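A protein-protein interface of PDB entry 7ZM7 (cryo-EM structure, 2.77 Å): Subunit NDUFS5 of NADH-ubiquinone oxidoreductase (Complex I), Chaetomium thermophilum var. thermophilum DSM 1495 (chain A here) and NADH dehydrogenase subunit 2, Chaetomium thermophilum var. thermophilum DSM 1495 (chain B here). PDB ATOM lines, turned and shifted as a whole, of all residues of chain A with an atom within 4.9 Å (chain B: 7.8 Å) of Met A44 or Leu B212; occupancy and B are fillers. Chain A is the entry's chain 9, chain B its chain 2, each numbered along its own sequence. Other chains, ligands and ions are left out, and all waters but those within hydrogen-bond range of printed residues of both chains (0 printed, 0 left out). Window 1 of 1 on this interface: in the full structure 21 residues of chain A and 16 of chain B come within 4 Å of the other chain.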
ATOM      1  N   TRP A  18     -19.624  17.142  17.338  1.00  0.00           N
ATOM      2  CA  TRP A  18     -19.862  17.755  16.011  1.00  0.00           C
ATOM      3  C   TRP A  18     -19.883  16.708  14.898  1.00  0.00           C
ATOM      4  O   TRP A  18     -20.697  16.839  13.987  1.00  0.00           O
ATOM      5  CB  TRP A  18     -18.755  18.781  15.760  1.00  0.00           C
ATOM      6  CG  TRP A  18     -18.864  19.450  14.429  1.00  0.00           C
ATOM      7  CD1 TRP A  18     -18.022  19.313  13.367  1.00  0.00           C
ATOM      8  CD2 TRP A  18     -19.906  20.343  14.007  1.00  0.00           C
ATOM      9  NE1 TRP A  18     -18.460  20.074  12.319  1.00  0.00           N
ATOM     10  CE2 TRP A  18     -19.611  20.718  12.681  1.00  0.00           C
ATOM     11  CE3 TRP A  18     -21.047  20.866  14.620  1.00  0.00           C
ATOM     12  CZ2 TRP A  18     -20.423  21.589  11.959  1.00  0.00           C
ATOM     13  CZ3 TRP A  18     -21.846  21.730  13.907  1.00  0.00           C
ATOM     14  CH2 TRP A  18     -21.536  22.084  12.596  1.00  0.00           C
ATOM     15  N   LEU A  21     -22.874  14.735  15.104  1.00  0.00           N
ATOM     16  CA  LEU A  21     -24.004  15.538  14.598  1.00  0.00           C
ATOM     17  C   LEU A  21     -23.900  15.603  13.082  1.00  0.00           C
ATOM     18  O   LEU A  21     -24.946  15.537  12.432  1.00  0.00           O
ATOM     19  CB  LEU A  21     -23.913  16.944  15.187  1.00  0.00           C
ATOM     20  CG  LEU A  21     -24.957  17.936  14.680  1.00  0.00           C
ATOM     21  CD1 LEU A  21     -26.358  17.432  14.967  1.00  0.00           C
ATOM     22  CD2 LEU A  21     -24.741  19.302  15.297  1.00  0.00           C
ATOM     23  N   CYS A  40     -31.494  14.335  14.576  1.00  0.00           N
ATOM     24  CA  CYS A  40     -30.332  15.150  14.862  1.00  0.00           C
ATOM     25  C   CYS A  40     -30.586  16.150  15.972  1.00  0.00           C
ATOM     26  O   CYS A  40     -29.648  16.826  16.396  1.00  0.00           O
ATOM     27  CB  CYS A  40     -29.921  15.900  13.598  1.00  0.00           C
ATOM     28  SG  CYS A  40     -29.714  14.871  12.173  1.00  0.00           S
ATOM     29  N   ILE A  41     -31.829  16.286  16.419  1.00  0.00           N
ATOM     30  CA  ILE A  41     -32.204  17.230  17.468  1.00  0.00           C
ATOM     31  C   ILE A  41     -31.477  16.913  18.768  1.00  0.00           C
ATOM     32  O   ILE A  41     -30.752  17.777  19.279  1.00  0.00           O
ATOM     33  CB  ILE A  41     -33.719  17.240  17.693  1.00  0.00           C
ATOM     34  CG1 ILE A  41     -34.467  17.305  16.368  1.00  0.00           C
ATOM     35  CG2 ILE A  41     -34.101  18.371  18.600  1.00  0.00           C
ATOM     36  CD1 ILE A  41     -34.421  18.622  15.718  1.00  0.00           C
ATOM     37  N   PRO A  42     -31.624  15.714  19.346  1.00  0.00           N
ATOM     38  CA  PRO A  42     -30.896  15.443  20.589  1.00  0.00           C
ATOM     39  C   PRO A  42     -29.396  15.430  20.382  1.00  0.00           C
ATOM     40  O   PRO A  42     -28.652  15.747  21.312  1.00  0.00           O
ATOM     41  CB  PRO A  42     -31.420  14.069  21.021  1.00  0.00           C
ATOM     42  CG  PRO A  42     -32.222  13.557  19.904  1.00  0.00           C
ATOM     43  CD  PRO A  42     -32.153  14.469  18.762  1.00  0.00           C
ATOM     44  N   VAL A  43     -28.940  15.064  19.187  1.00  0.00           N
ATOM     45  CA  VAL A  43     -27.516  15.056  18.896  1.00  0.00           C
ATOM     46  C   VAL A  43     -26.983  16.482  18.824  1.00  0.00           C
ATOM     47  O   VAL A  43     -25.879  16.770  19.292  1.00  0.00           O
ATOM     48  CB  VAL A  43     -27.262  14.254  17.605  1.00  0.00           C
ATOM     49  CG1 VAL A  43     -25.795  14.001  17.383  1.00  0.00           C
ATOM     50  CG2 VAL A  43     -28.002  12.949  17.674  1.00  0.00           C
ATOM     51  N   MET A  44     -27.771  17.401  18.262  1.00  0.00           N
ATOM     52  CA  MET A  44     -27.424  18.819  18.269  1.00  0.00           C
ATOM     53  C   MET A  44     -27.437  19.413  19.672  1.00  0.00           C
ATOM     54  O   MET A  44     -26.663  20.326  19.960  1.00  0.00           O
ATOM     55  CB  MET A  44     -28.380  19.590  17.364  1.00  0.00           C
ATOM     56  CG  MET A  44     -27.781  20.789  16.678  1.00  0.00           C
ATOM     57  SD  MET A  44     -28.968  21.928  15.957  1.00  0.00           S
ATOM     58  CE  MET A  44     -29.903  22.386  17.398  1.00  0.00           C
ATOM     59  N   GLU A  45     -28.328  18.946  20.546  1.00  0.00           N
ATOM     60  CA  GLU A  45     -28.354  19.463  21.909  1.00  0.00           C
ATOM     61  C   GLU A  45     -27.064  19.141  22.638  1.00  0.00           C
ATOM     62  O   GLU A  45     -26.542  19.969  23.388  1.00  0.00           O
ATOM     63  CB  GLU A  45     -29.544  18.893  22.668  1.00  0.00           C
ATOM     64  CG  GLU A  45     -30.866  19.516  22.312  1.00  0.00           C
ATOM     65  CD  GLU A  45     -32.021  18.913  23.090  1.00  0.00           C
ATOM     66  OE1 GLU A  45     -32.465  17.802  22.733  1.00  0.00           O
ATOM     67  OE2 GLU A  45     -32.484  19.547  24.062  1.00  0.00           O
ATOM     68  N   ASP A  46     -26.539  17.935  22.433  1.00  0.00           N
ATOM     69  CA  ASP A  46     -25.299  17.548  23.078  1.00  0.00           C
ATOM     70  C   ASP A  46     -24.137  18.382  22.579  1.00  0.00           C
ATOM     71  O   ASP A  46     -23.245  18.740  23.353  1.00  0.00           O
ATOM     72  CB  ASP A  46     -25.033  16.070  22.856  1.00  0.00           C
ATOM     73  CG  ASP A  46     -26.157  15.210  23.346  1.00  0.00           C
ATOM     74  OD1 ASP A  46     -26.824  15.611  24.315  1.00  0.00           O
ATOM     75  OD2 ASP A  46     -26.383  14.138  22.761  1.00  0.00           O
ATOM     76  N   TYR A  47     -24.129  18.700  21.287  1.00  0.00           N
ATOM     77  CA  TYR A  47     -23.100  19.580  20.765  1.00  0.00           C
ATOM     78  C   TYR A  47     -23.195  20.956  21.404  1.00  0.00           C
ATOM     79  O   TYR A  47     -22.192  21.514  21.851  1.00  0.00           O
ATOM     80  CB  TYR A  47     -23.205  19.685  19.247  1.00  0.00           C
ATOM     81  CG  TYR A  47     -22.218  20.680  18.695  1.00  0.00           C
ATOM     82  CD1 TYR A  47     -20.862  20.472  18.841  1.00  0.00           C
ATOM     83  CD2 TYR A  47     -22.639  21.845  18.090  1.00  0.00           C
ATOM     84  CE1 TYR A  47     -19.963  21.365  18.372  1.00  0.00           C
ATOM     85  CE2 TYR A  47     -21.741  22.743  17.620  1.00  0.00           C
ATOM     86  CZ  TYR A  47     -20.402  22.498  17.759  1.00  0.00           C
ATOM     87  OH  TYR A  47     -19.488  23.391  17.283  1.00  0.00           O
ATOM     88  N   TYR A  48     -24.399  21.493  21.556  1.00  0.00           N
ATOM     89  CA  TYR A  48     -24.531  22.858  22.120  1.00  0.00           C
ATOM     90  C   TYR A  48     -24.203  22.811  23.608  1.00  0.00           C
ATOM     91  O   TYR A  48     -23.721  23.814  24.141  1.00  0.00           O
ATOM     92  CB  TYR A  48     -25.900  23.454  21.819  1.00  0.00           C
ATOM     93  CG  TYR A  48     -26.048  24.168  20.500  1.00  0.00           C
ATOM     94  CD1 TYR A  48     -25.199  25.198  20.132  1.00  0.00           C
ATOM     95  CD2 TYR A  48     -27.079  23.840  19.640  1.00  0.00           C
ATOM     96  CE1 TYR A  48     -25.351  25.864  18.928  1.00  0.00           C
ATOM     97  CE2 TYR A  48     -27.246  24.496  18.435  1.00  0.00           C
ATOM     98  CZ  TYR A  48     -26.382  25.510  18.076  1.00  0.00           C
ATOM     99  OH  TYR A  48     -26.564  26.142  16.882  1.00  0.00           O
ATOM    100  N   LEU B 197     -21.314  34.725  15.575  1.00  0.00           N
ATOM    101  CA  LEU B 197     -21.683  33.447  14.993  1.00  0.00           C
ATOM    102  C   LEU B 197     -20.809  32.328  15.526  1.00  0.00           C
ATOM    103  O   LEU B 197     -21.320  31.316  16.008  1.00  0.00           O
ATOM    104  CB  LEU B 197     -21.579  33.527  13.476  1.00  0.00           C
ATOM    105  CG  LEU B 197     -22.812  34.065  12.779  1.00  0.00           C
ATOM    106  CD1 LEU B 197     -22.441  34.481  11.387  1.00  0.00           C
ATOM    107  CD2 LEU B 197     -23.887  33.021  12.762  1.00  0.00           C
ATOM    108  N   ASN B 200     -21.067  31.243  19.307  1.00  0.00           N
ATOM    109  CA  ASN B 200     -22.296  30.553  19.762  1.00  0.00           C
ATOM    110  C   ASN B 200     -22.410  29.191  19.102  1.00  0.00           C
ATOM    111  O   ASN B 200     -23.082  28.336  19.663  1.00  0.00           O
ATOM    112  CB  ASN B 200     -23.529  31.387  19.456  1.00  0.00           C
ATOM    113  CG  ASN B 200     -23.746  32.524  20.433  1.00  0.00           C
ATOM    114  OD1 ASN B 200     -23.991  32.295  21.611  1.00  0.00           O
ATOM    115  ND2 ASN B 200     -23.683  33.752  19.951  1.00  0.00           N
ATOM    116  N   SER B 201     -21.748  28.997  17.970  1.00  0.00           N
ATOM    117  CA  SER B 201     -21.853  27.746  17.190  1.00  0.00           C
ATOM    118  C   SER B 201     -20.562  26.933  17.222  1.00  0.00           C
ATOM    119  O   SER B 201     -20.607  25.799  16.761  1.00  0.00           O
ATOM    120  CB  SER B 201     -22.182  28.128  15.808  1.00  0.00           C
ATOM    121  OG  SER B 201     -21.135  28.888  15.242  1.00  0.00           O
ATOM    122  N   GLY B 202     -19.441  27.502  17.662  1.00  0.00           N
ATOM    123  CA  GLY B 202     -18.188  26.783  17.610  1.00  0.00           C
ATOM    124  C   GLY B 202     -17.629  26.512  16.237  1.00  0.00           C
ATOM    125  O   GLY B 202     -16.627  25.814  16.126  1.00  0.00           O
ATOM    126  N   THR B 203     -18.253  27.065  15.202  1.00  0.00           N
ATOM    127  CA  THR B 203     -17.829  26.773  13.813  1.00  0.00           C
ATOM    128  C   THR B 203     -17.645  28.059  13.021  1.00  0.00           C
ATOM    129  O   THR B 203     -18.296  29.048  13.376  1.00  0.00           O
ATOM    130  CB  THR B 203     -18.854  25.890  13.086  1.00  0.00           C
ATOM    131  OG1 THR B 203     -18.339  25.587  11.788  1.00  0.00           O
ATOM    132  CG2 THR B 203     -20.230  26.505  12.965  1.00  0.00           C
ATOM    133  N   SER B 205     -17.382  27.542   9.518  1.00  0.00           N
ATOM    134  CA  SER B 205     -17.880  27.022   8.217  1.00  0.00           C
ATOM    135  C   SER B 205     -19.359  27.360   8.014  1.00  0.00           C
ATOM    136  O   SER B 205     -20.152  27.095   8.923  1.00  0.00           O
ATOM    137  CB  SER B 205     -17.672  25.537   8.145  1.00  0.00           C
ATOM    138  OG  SER B 205     -18.478  24.856   9.089  1.00  0.00           O
ATOM    139  N   LEU B 206     -19.710  27.916   6.856  1.00  0.00           N
ATOM    140  CA  LEU B 206     -21.110  28.294   6.547  1.00  0.00           C
ATOM    141  C   LEU B 206     -22.005  27.056   6.484  1.00  0.00           C
ATOM    142  O   LEU B 206     -23.121  27.130   6.996  1.00  0.00           O
ATOM    143  CB  LEU B 206     -21.131  29.063   5.225  1.00  0.00           C
ATOM    144  CG  LEU B 206     -20.590  30.488   5.290  1.00  0.00           C
ATOM    145  CD1 LEU B 206     -20.843  31.217   3.981  1.00  0.00           C
ATOM    146  CD2 LEU B 206     -21.213  31.244   6.452  1.00  0.00           C
ATOM    147  N   ASP B 207     -21.524  25.964   5.892  1.00  0.00           N
ATOM    148  CA  ASP B 207     -22.327  24.719   5.764  1.00  0.00           C
ATOM    149  C   ASP B 207     -22.695  24.161   7.143  1.00  0.00           C
ATOM    150  O   ASP B 207     -23.845  23.735   7.285  1.00  0.00           O
ATOM    151  CB  ASP B 207     -21.644  23.700   4.858  1.00  0.00           C
ATOM    152  CG  ASP B 207     -22.310  23.584   3.496  1.00  0.00           C
ATOM    153  OD1 ASP B 207     -21.750  22.896   2.621  1.00  0.00           O
ATOM    154  OD2 ASP B 207     -23.388  24.184   3.320  1.00  0.00           O
ATOM    155  N   GLY B 208     -21.782  24.184   8.120  1.00  0.00           N
ATOM    156  CA  GLY B 208     -22.150  23.761   9.484  1.00  0.00           C
ATOM    157  C   GLY B 208     -23.227  24.647  10.080  1.00  0.00           C
ATOM    158  O   GLY B 208     -24.144  24.094  10.687  1.00  0.00           O
ATOM    159  N   LEU B 209     -23.127  25.962   9.899  1.00  0.00           N
ATOM    160  CA  LEU B 209     -24.151  26.925  10.370  1.00  0.00           C
ATOM    161  C   LEU B 209     -25.471  26.663   9.650  1.00  0.00           C
ATOM    162  O   LEU B 209     -26.514  26.781  10.303  1.00  0.00           O
ATOM    163  CB  LEU B 209     -23.648  28.332  10.049  1.00  0.00           C
ATOM    164  CG  LEU B 209     -22.669  28.925  11.060  1.00  0.00           C
ATOM    165  CD1 LEU B 209     -22.002  30.172  10.501  1.00  0.00           C
ATOM    166  CD2 LEU B 209     -23.370  29.238  12.371  1.00  0.00           C
ATOM    167  N   TYR B 210     -25.414  26.344   8.355  1.00  0.00           N
ATOM    168  CA  TYR B 210     -26.625  26.034   7.557  1.00  0.00           C
ATOM    169  C   TYR B 210     -27.308  24.791   8.124  1.00  0.00           C
ATOM    170  O   TYR B 210     -28.544  24.784   8.182  1.00  0.00           O
ATOM    171  CB  TYR B 210     -26.256  25.825   6.086  1.00  0.00           C
ATOM    172  CG  TYR B 210     -25.793  27.053   5.349  1.00  0.00           C
ATOM    173  CD1 TYR B 210     -26.163  28.321   5.761  1.00  0.00           C
ATOM    174  CD2 TYR B 210     -24.988  26.943   4.229  1.00  0.00           C
ATOM    175  CE1 TYR B 210     -25.739  29.450   5.081  1.00  0.00           C
ATOM    176  CE2 TYR B 210     -24.554  28.060   3.539  1.00  0.00           C
ATOM    177  CZ  TYR B 210     -24.936  29.318   3.964  1.00  0.00           C
ATOM    178  OH  TYR B 210     -24.517  30.422   3.284  1.00  0.00           O
ATOM    179  N   ILE B 211     -26.530  23.784   8.526  1.00  0.00           N
ATOM    180  CA  ILE B 211     -27.094  22.520   9.088  1.00  0.00           C
ATOM    181  C   ILE B 211     -27.625  22.760  10.510  1.00  0.00           C
ATOM    182  O   ILE B 211     -28.662  22.195  10.852  1.00  0.00           O
ATOM    183  CB  ILE B 211     -26.025  21.409   9.039  1.00  0.00           C
ATOM    184  CG1 ILE B 211     -25.752  20.953   7.605  1.00  0.00           C
ATOM    185  CG2 ILE B 211     -26.369  20.236   9.941  1.00  0.00           C
ATOM    186  CD1 ILE B 211     -24.596  19.998   7.490  1.00  0.00           C
ATOM    187  N   LEU B 212     -26.944  23.576  11.307  1.00  0.00           N
ATOM    188  CA  LEU B 212     -27.442  23.909  12.665  1.00  0.00           C
ATOM    189  C   LEU B 212     -28.766  24.657  12.516  1.00  0.00           C
ATOM    190  O   LEU B 212     -29.643  24.443  13.352  1.00  0.00           O
ATOM    191  CB  LEU B 212     -26.389  24.740  13.404  1.00  0.00           C
ATOM    192  CG  LEU B 212     -25.145  23.992  13.872  1.00  0.00           C
ATOM    193  CD1 LEU B 212     -24.136  24.962  14.468  1.00  0.00           C
ATOM    194  CD2 LEU B 212     -25.510  22.919  14.880  1.00  0.00           C
ATOM    195  N   ASN B 213     -28.918  25.467  11.475  1.00  0.00           N
ATOM    196  CA  ASN B 213     -30.187  26.186  11.199  1.00  0.00           C
ATOM    197  C   ASN B 213     -31.204  25.204  10.622  1.00  0.00           C
ATOM    198  O   ASN B 213     -32.391  25.359  10.921  1.00  0.00           O
ATOM    199  CB  ASN B 213     -29.929  27.381  10.278  1.00  0.00           C
ATOM    200  CG  ASN B 213     -31.149  27.886   9.537  1.00  0.00           C
ATOM    201  OD1 ASN B 213     -32.027  28.512  10.123  1.00  0.00           O
ATOM    202  ND2 ASN B 213     -31.200  27.638   8.238  1.00  0.00           N
ATOM    203  N   SER B 214     -30.758  24.260   9.800  1.00  0.00           N
ATOM    204  CA  SER B 214     -31.650  23.236   9.196  1.00  0.00           C
ATOM    205  C   SER B 214     -32.278  22.365  10.282  1.00  0.00           C
ATOM    206  O   SER B 214     -33.474  22.119  10.202  1.00  0.00           O
ATOM    207  CB  SER B 214     -30.876  22.388   8.221  1.00  0.00           C
ATOM    208  OG  SER B 214     -31.741  21.649   7.379  1.00  0.00           O
ATOM    209  N   ILE B 215     -31.520  22.008  11.312  1.00  0.00           N
ATOM    210  CA  ILE B 215     -32.026  21.062  12.351  1.00  0.00           C
ATOM    211  C   ILE B 215     -32.941  21.827  13.304  1.00  0.00           C
ATOM    212  O   ILE B 215     -33.949  21.254  13.729  1.00  0.00           O
ATOM    213  CB  ILE B 215     -30.878  20.297  13.036  1.00  0.00           C
ATOM    214  CG1 ILE B 215     -30.099  19.440  12.037  1.00  0.00           C
ATOM    215  CG2 ILE B 215     -31.368  19.473  14.213  1.00  0.00           C
ATOM    216  CD1 ILE B 215     -28.715  19.077  12.503  1.00  0.00           C
ATOM    217  N   SER B 216     -32.634  23.094  13.551  1.00  0.00           N
ATOM    218  CA  SER B 216     -33.510  23.915  14.375  1.00  0.00           C
ATOM    219  C   SER B 216     -34.876  24.161  13.741  1.00  0.00           C
ATOM    220  O   SER B 216     -35.879  24.203  14.456  1.00  0.00           O
ATOM    221  CB  SER B 216     -32.848  25.253  14.644  1.00  0.00           C
ATOM    222  OG  SER B 216     -32.874  26.035  13.461  1.00  0.00           O
ATOM    223  N   ASP B 217     -34.936  24.321  12.422  1.00  0.00           N
ATOM    224  CA  ASP B 217     -36.178  24.622  11.715  1.00  0.00           C
ATOM    225  C   ASP B 217     -37.077  23.387  11.714  1.00  0.00           C
ATOM    226  O   ASP B 217     -37.183  22.642  10.740  1.00  0.00           O
ATOM    227  CB  ASP B 217     -35.874  25.094  10.300  1.00  0.00           C
ATOM    228  CG  ASP B 217     -37.088  25.682   9.603  1.00  0.00           C
ATOM    229  OD1 ASP B 217     -38.089  25.968  10.292  1.00  0.00           O
ATOM    230  OD2 ASP B 217     -37.046  25.847   8.366  1.00  0.00           O
ATOM    231  N   SER B 233     -34.389  22.337  23.749  1.00  0.00           N
ATOM    232  CA  SER B 233     -35.197  23.326  24.450  1.00  0.00           C
ATOM    233  C   SER B 233     -34.303  24.277  25.230  1.00  0.00           C
ATOM    234  O   SER B 233     -34.629  25.445  25.421  1.00  0.00           O
ATOM    235  CB  SER B 233     -36.188  22.638  25.390  1.00  0.00           C
ATOM    236  OG  SER B 233     -37.033  21.752  24.677  1.00  0.00           O
ATOM    237  N   TYR B 235     -31.322  25.245  24.313  1.00  0.00           N
ATOM    238  CA  TYR B 235     -30.436  26.054  23.435  1.00  0.00           C
ATOM    239  C   TYR B 235     -31.176  26.506  22.180  1.00  0.00           C
ATOM    240  O   TYR B 235     -30.968  25.910  21.121  1.00  0.00           O
ATOM    241  CB  TYR B 235     -29.198  25.256  23.028  1.00  0.00           C
ATOM    242  CG  TYR B 235     -28.214  24.994  24.136  1.00  0.00           C
ATOM    243  CD1 TYR B 235     -28.287  23.839  24.896  1.00  0.00           C
ATOM    244  CD2 TYR B 235     -27.208  25.900  24.418  1.00  0.00           C
ATOM    245  CE1 TYR B 235     -27.389  23.594  25.918  1.00  0.00           C
ATOM    246  CE2 TYR B 235     -26.293  25.664  25.428  1.00  0.00           C
ATOM    247  CZ  TYR B 235     -26.388  24.509  26.182  1.00  0.00           C
ATOM    248  OH  TYR B 235     -25.488  24.277  27.175  1.00  0.00           O
ATOM    249  N   LYS B 236     -32.013  27.527  22.295  1.00  0.00           N
ATOM    250  CA  LYS B 236     -32.706  28.098  21.117  1.00  0.00           C
ATOM    251  C   LYS B 236     -31.647  28.680  20.193  1.00  0.00           C
ATOM    252  O   LYS B 236     -30.755  29.360  20.710  1.00  0.00           O
ATOM    253  CB  LYS B 236     -33.572  29.264  21.593  1.00  0.00           C
ATOM    254  CG  LYS B 236     -34.427  28.977  22.821  1.00  0.00           C
ATOM    255  CD  LYS B 236     -35.451  27.881  22.608  1.00  0.00           C
ATOM    256  CE  LYS B 236     -36.596  28.300  21.711  1.00  0.00           C
ATOM    257  NZ  LYS B 236     -37.363  29.428  22.290  1.00  0.00           N
ATOM    258  N   PRO B 237     -31.708  28.495  18.861  1.00  0.00           N
ATOM    259  CA  PRO B 237     -30.717  29.134  17.987  1.00  0.00           C
ATOM    260  C   PRO B 237     -31.044  30.586  17.599  1.00  0.00           C
ATOM    261  O   PRO B 237     -30.918  30.903  16.449  1.00  0.00           O
ATOM    262  CB  PRO B 237     -30.807  28.212  16.767  1.00  0.00           C
ATOM    263  CG  PRO B 237     -32.254  27.781  16.716  1.00  0.00           C
ATOM    264  CD  PRO B 237     -32.680  27.661  18.163  1.00  0.00           C
ATOM    265  N   TYR B 239     -29.384  33.208  17.997  1.00  0.00           N
ATOM    266  CA  TYR B 239     -28.181  33.934  17.553  1.00  0.00           C
ATOM    267  C   TYR B 239     -28.113  34.026  16.040  1.00  0.00           C
ATOM    268  O   TYR B 239     -27.664  35.061  15.591  1.00  0.00           O
ATOM    269  CB  TYR B 239     -26.928  33.246  18.100  1.00  0.00           C
ATOM    270  CG  TYR B 239     -26.595  31.895  17.520  1.00  0.00           C
ATOM    271  CD1 TYR B 239     -27.209  30.747  17.985  1.00  0.00           C
ATOM    272  CD2 TYR B 239     -25.644  31.763  16.522  1.00  0.00           C
ATOM    273  CE1 TYR B 239     -26.906  29.505  17.457  1.00  0.00           C
ATOM    274  CE2 TYR B 239     -25.333  30.530  15.979  1.00  0.00           C
ATOM    275  CZ  TYR B 239     -25.964  29.397  16.453  1.00  0.00           C
ATOM    276  OH  TYR B 239     -25.663  28.174  15.930  1.00  0.00           O
ATOM    277  N   LEU B 240     -28.507  32.991  15.298  1.00  0.00           N
ATOM    278  CA  LEU B 240     -28.307  33.019  13.836  1.00  0.00           C
ATOM    279  C   LEU B 240     -29.003  34.241  13.232  1.00  0.00           C
ATOM    280  O   LEU B 240     -28.368  34.942  12.452  1.00  0.00           O
ATOM    281  CB  LEU B 240     -28.812  31.709  13.242  1.00  0.00           C
ATOM    282  CG  LEU B 240     -28.632  31.583  11.731  1.00  0.00           C
ATOM    283  CD1 LEU B 240     -27.229  31.109  11.386  1.00  0.00           C
ATOM    284  CD2 LEU B 240     -29.676  30.662  11.128  1.00  0.00           C
ATOM    285  N   LEU B 306     -38.775  30.817  14.636  1.00  0.00           N
ATOM    286  CA  LEU B 306     -37.508  31.234  14.051  1.00  0.00           C
ATOM    287  C   LEU B 306     -37.737  32.279  12.965  1.00  0.00           C
ATOM    288  O   LEU B 306     -36.990  33.255  12.863  1.00  0.00           O
ATOM    289  CB  LEU B 306     -36.765  30.039  13.459  1.00  0.00           C
ATOM    290  CG  LEU B 306     -35.939  29.109  14.356  1.00  0.00           C
ATOM    291  CD1 LEU B 306     -34.774  29.797  15.072  1.00  0.00           C
ATOM    292  CD2 LEU B 306     -36.800  28.281  15.290  1.00  0.00           C
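Trp A18 touches Gly B208.
Trp A18 touches Leu B212 (CZ3 to CD2, 3.97 Å).
Leu A21 touches Leu B212 (CD2 to CD2, 3.7 Å).
Leu A21 touches Ile B215.
O of Ile B215 touches CD1 of Ile A41, 3.3 Å away.
CG2 of Ile B215 touches SD of Met A44, 3.9 Å away.
Tyr A47 touches Gly B202 (OH to CA, 3.6 Å).
Tyr A48 touches Asn B200.
Tyr A48 touches Leu B212.
Tyr A48 touches Tyr B235 (O to CE2, 3.4 Å).
Of the 11 printed residues of chain A, 8 touch a printed residue of chain B.
Hydrophobic or aromatic side chains of chain A within 4 Å of the printed part of chain B: Trp A18, Leu A21, Ile A41, Met A44, Tyr A47 and Tyr A48.
Along chain A the printed residues that touch a printed residue of chain B span positions 18 to 48.
Printed residues of chain B that touch a printed residue of chain A: Asn B200, Ser B201, Gly B202, Gly B208, Leu B212, Ile B215, Ser B233, Tyr B235 and Tyr B239.
OG of Ser B201 is in hydrogen-bond range of O of Leu B197 (2.6 Å).
The side-chain hydroxyl (OG) of Ser B201 sits at hydrogen-bond distance from the backbone carbonyl oxygen (O) of Thr B203, 3.4 Å away.
Leu B212 touches just these residues of chain A: Trp A18, Leu A21, Met A44 and Tyr A48.
Printed residues of chain A within 4 Å of Ser B233: Glu A45.
Of the printed residues of chain B, Leu A21 touches Leu B212 and Ile B215.
Printed residues of chain B within 4 Å of Glu A45: Ser B233.
Printed residues of chain A within 4 Å of Tyr B239: Tyr A48 (2.4 Å).
Leu B206 touches none of the printed residues of chain A.
Lys B236 touches none of the printed residues of chain A.
The nearest residue of chain B that does not touch Met A44 is Ser B216 (4.5 Å).
The nearest printed residue of chain A that does not touch Ser B233 is Ile A41 (6.5 Å).
OH of Tyr A48 lies within hydrogen-bond range of OH of Tyr B239 (2.4 Å).
The side-chain sulfur (SD) of Met A44 lies close to the backbone carbonyl oxygen (O) of Leu B212 (3.7 Å).
The side-chain hydroxyl (OH) of Tyr A47 lies within hydrogen-bond range of the backbone carbonyl oxygen (O) of Ser B201 (2.7 Å).
The backbone NH (N) of Ser B233 sits at hydrogen-bond distance from the side-chain carboxylate (OE2) of Glu A45.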
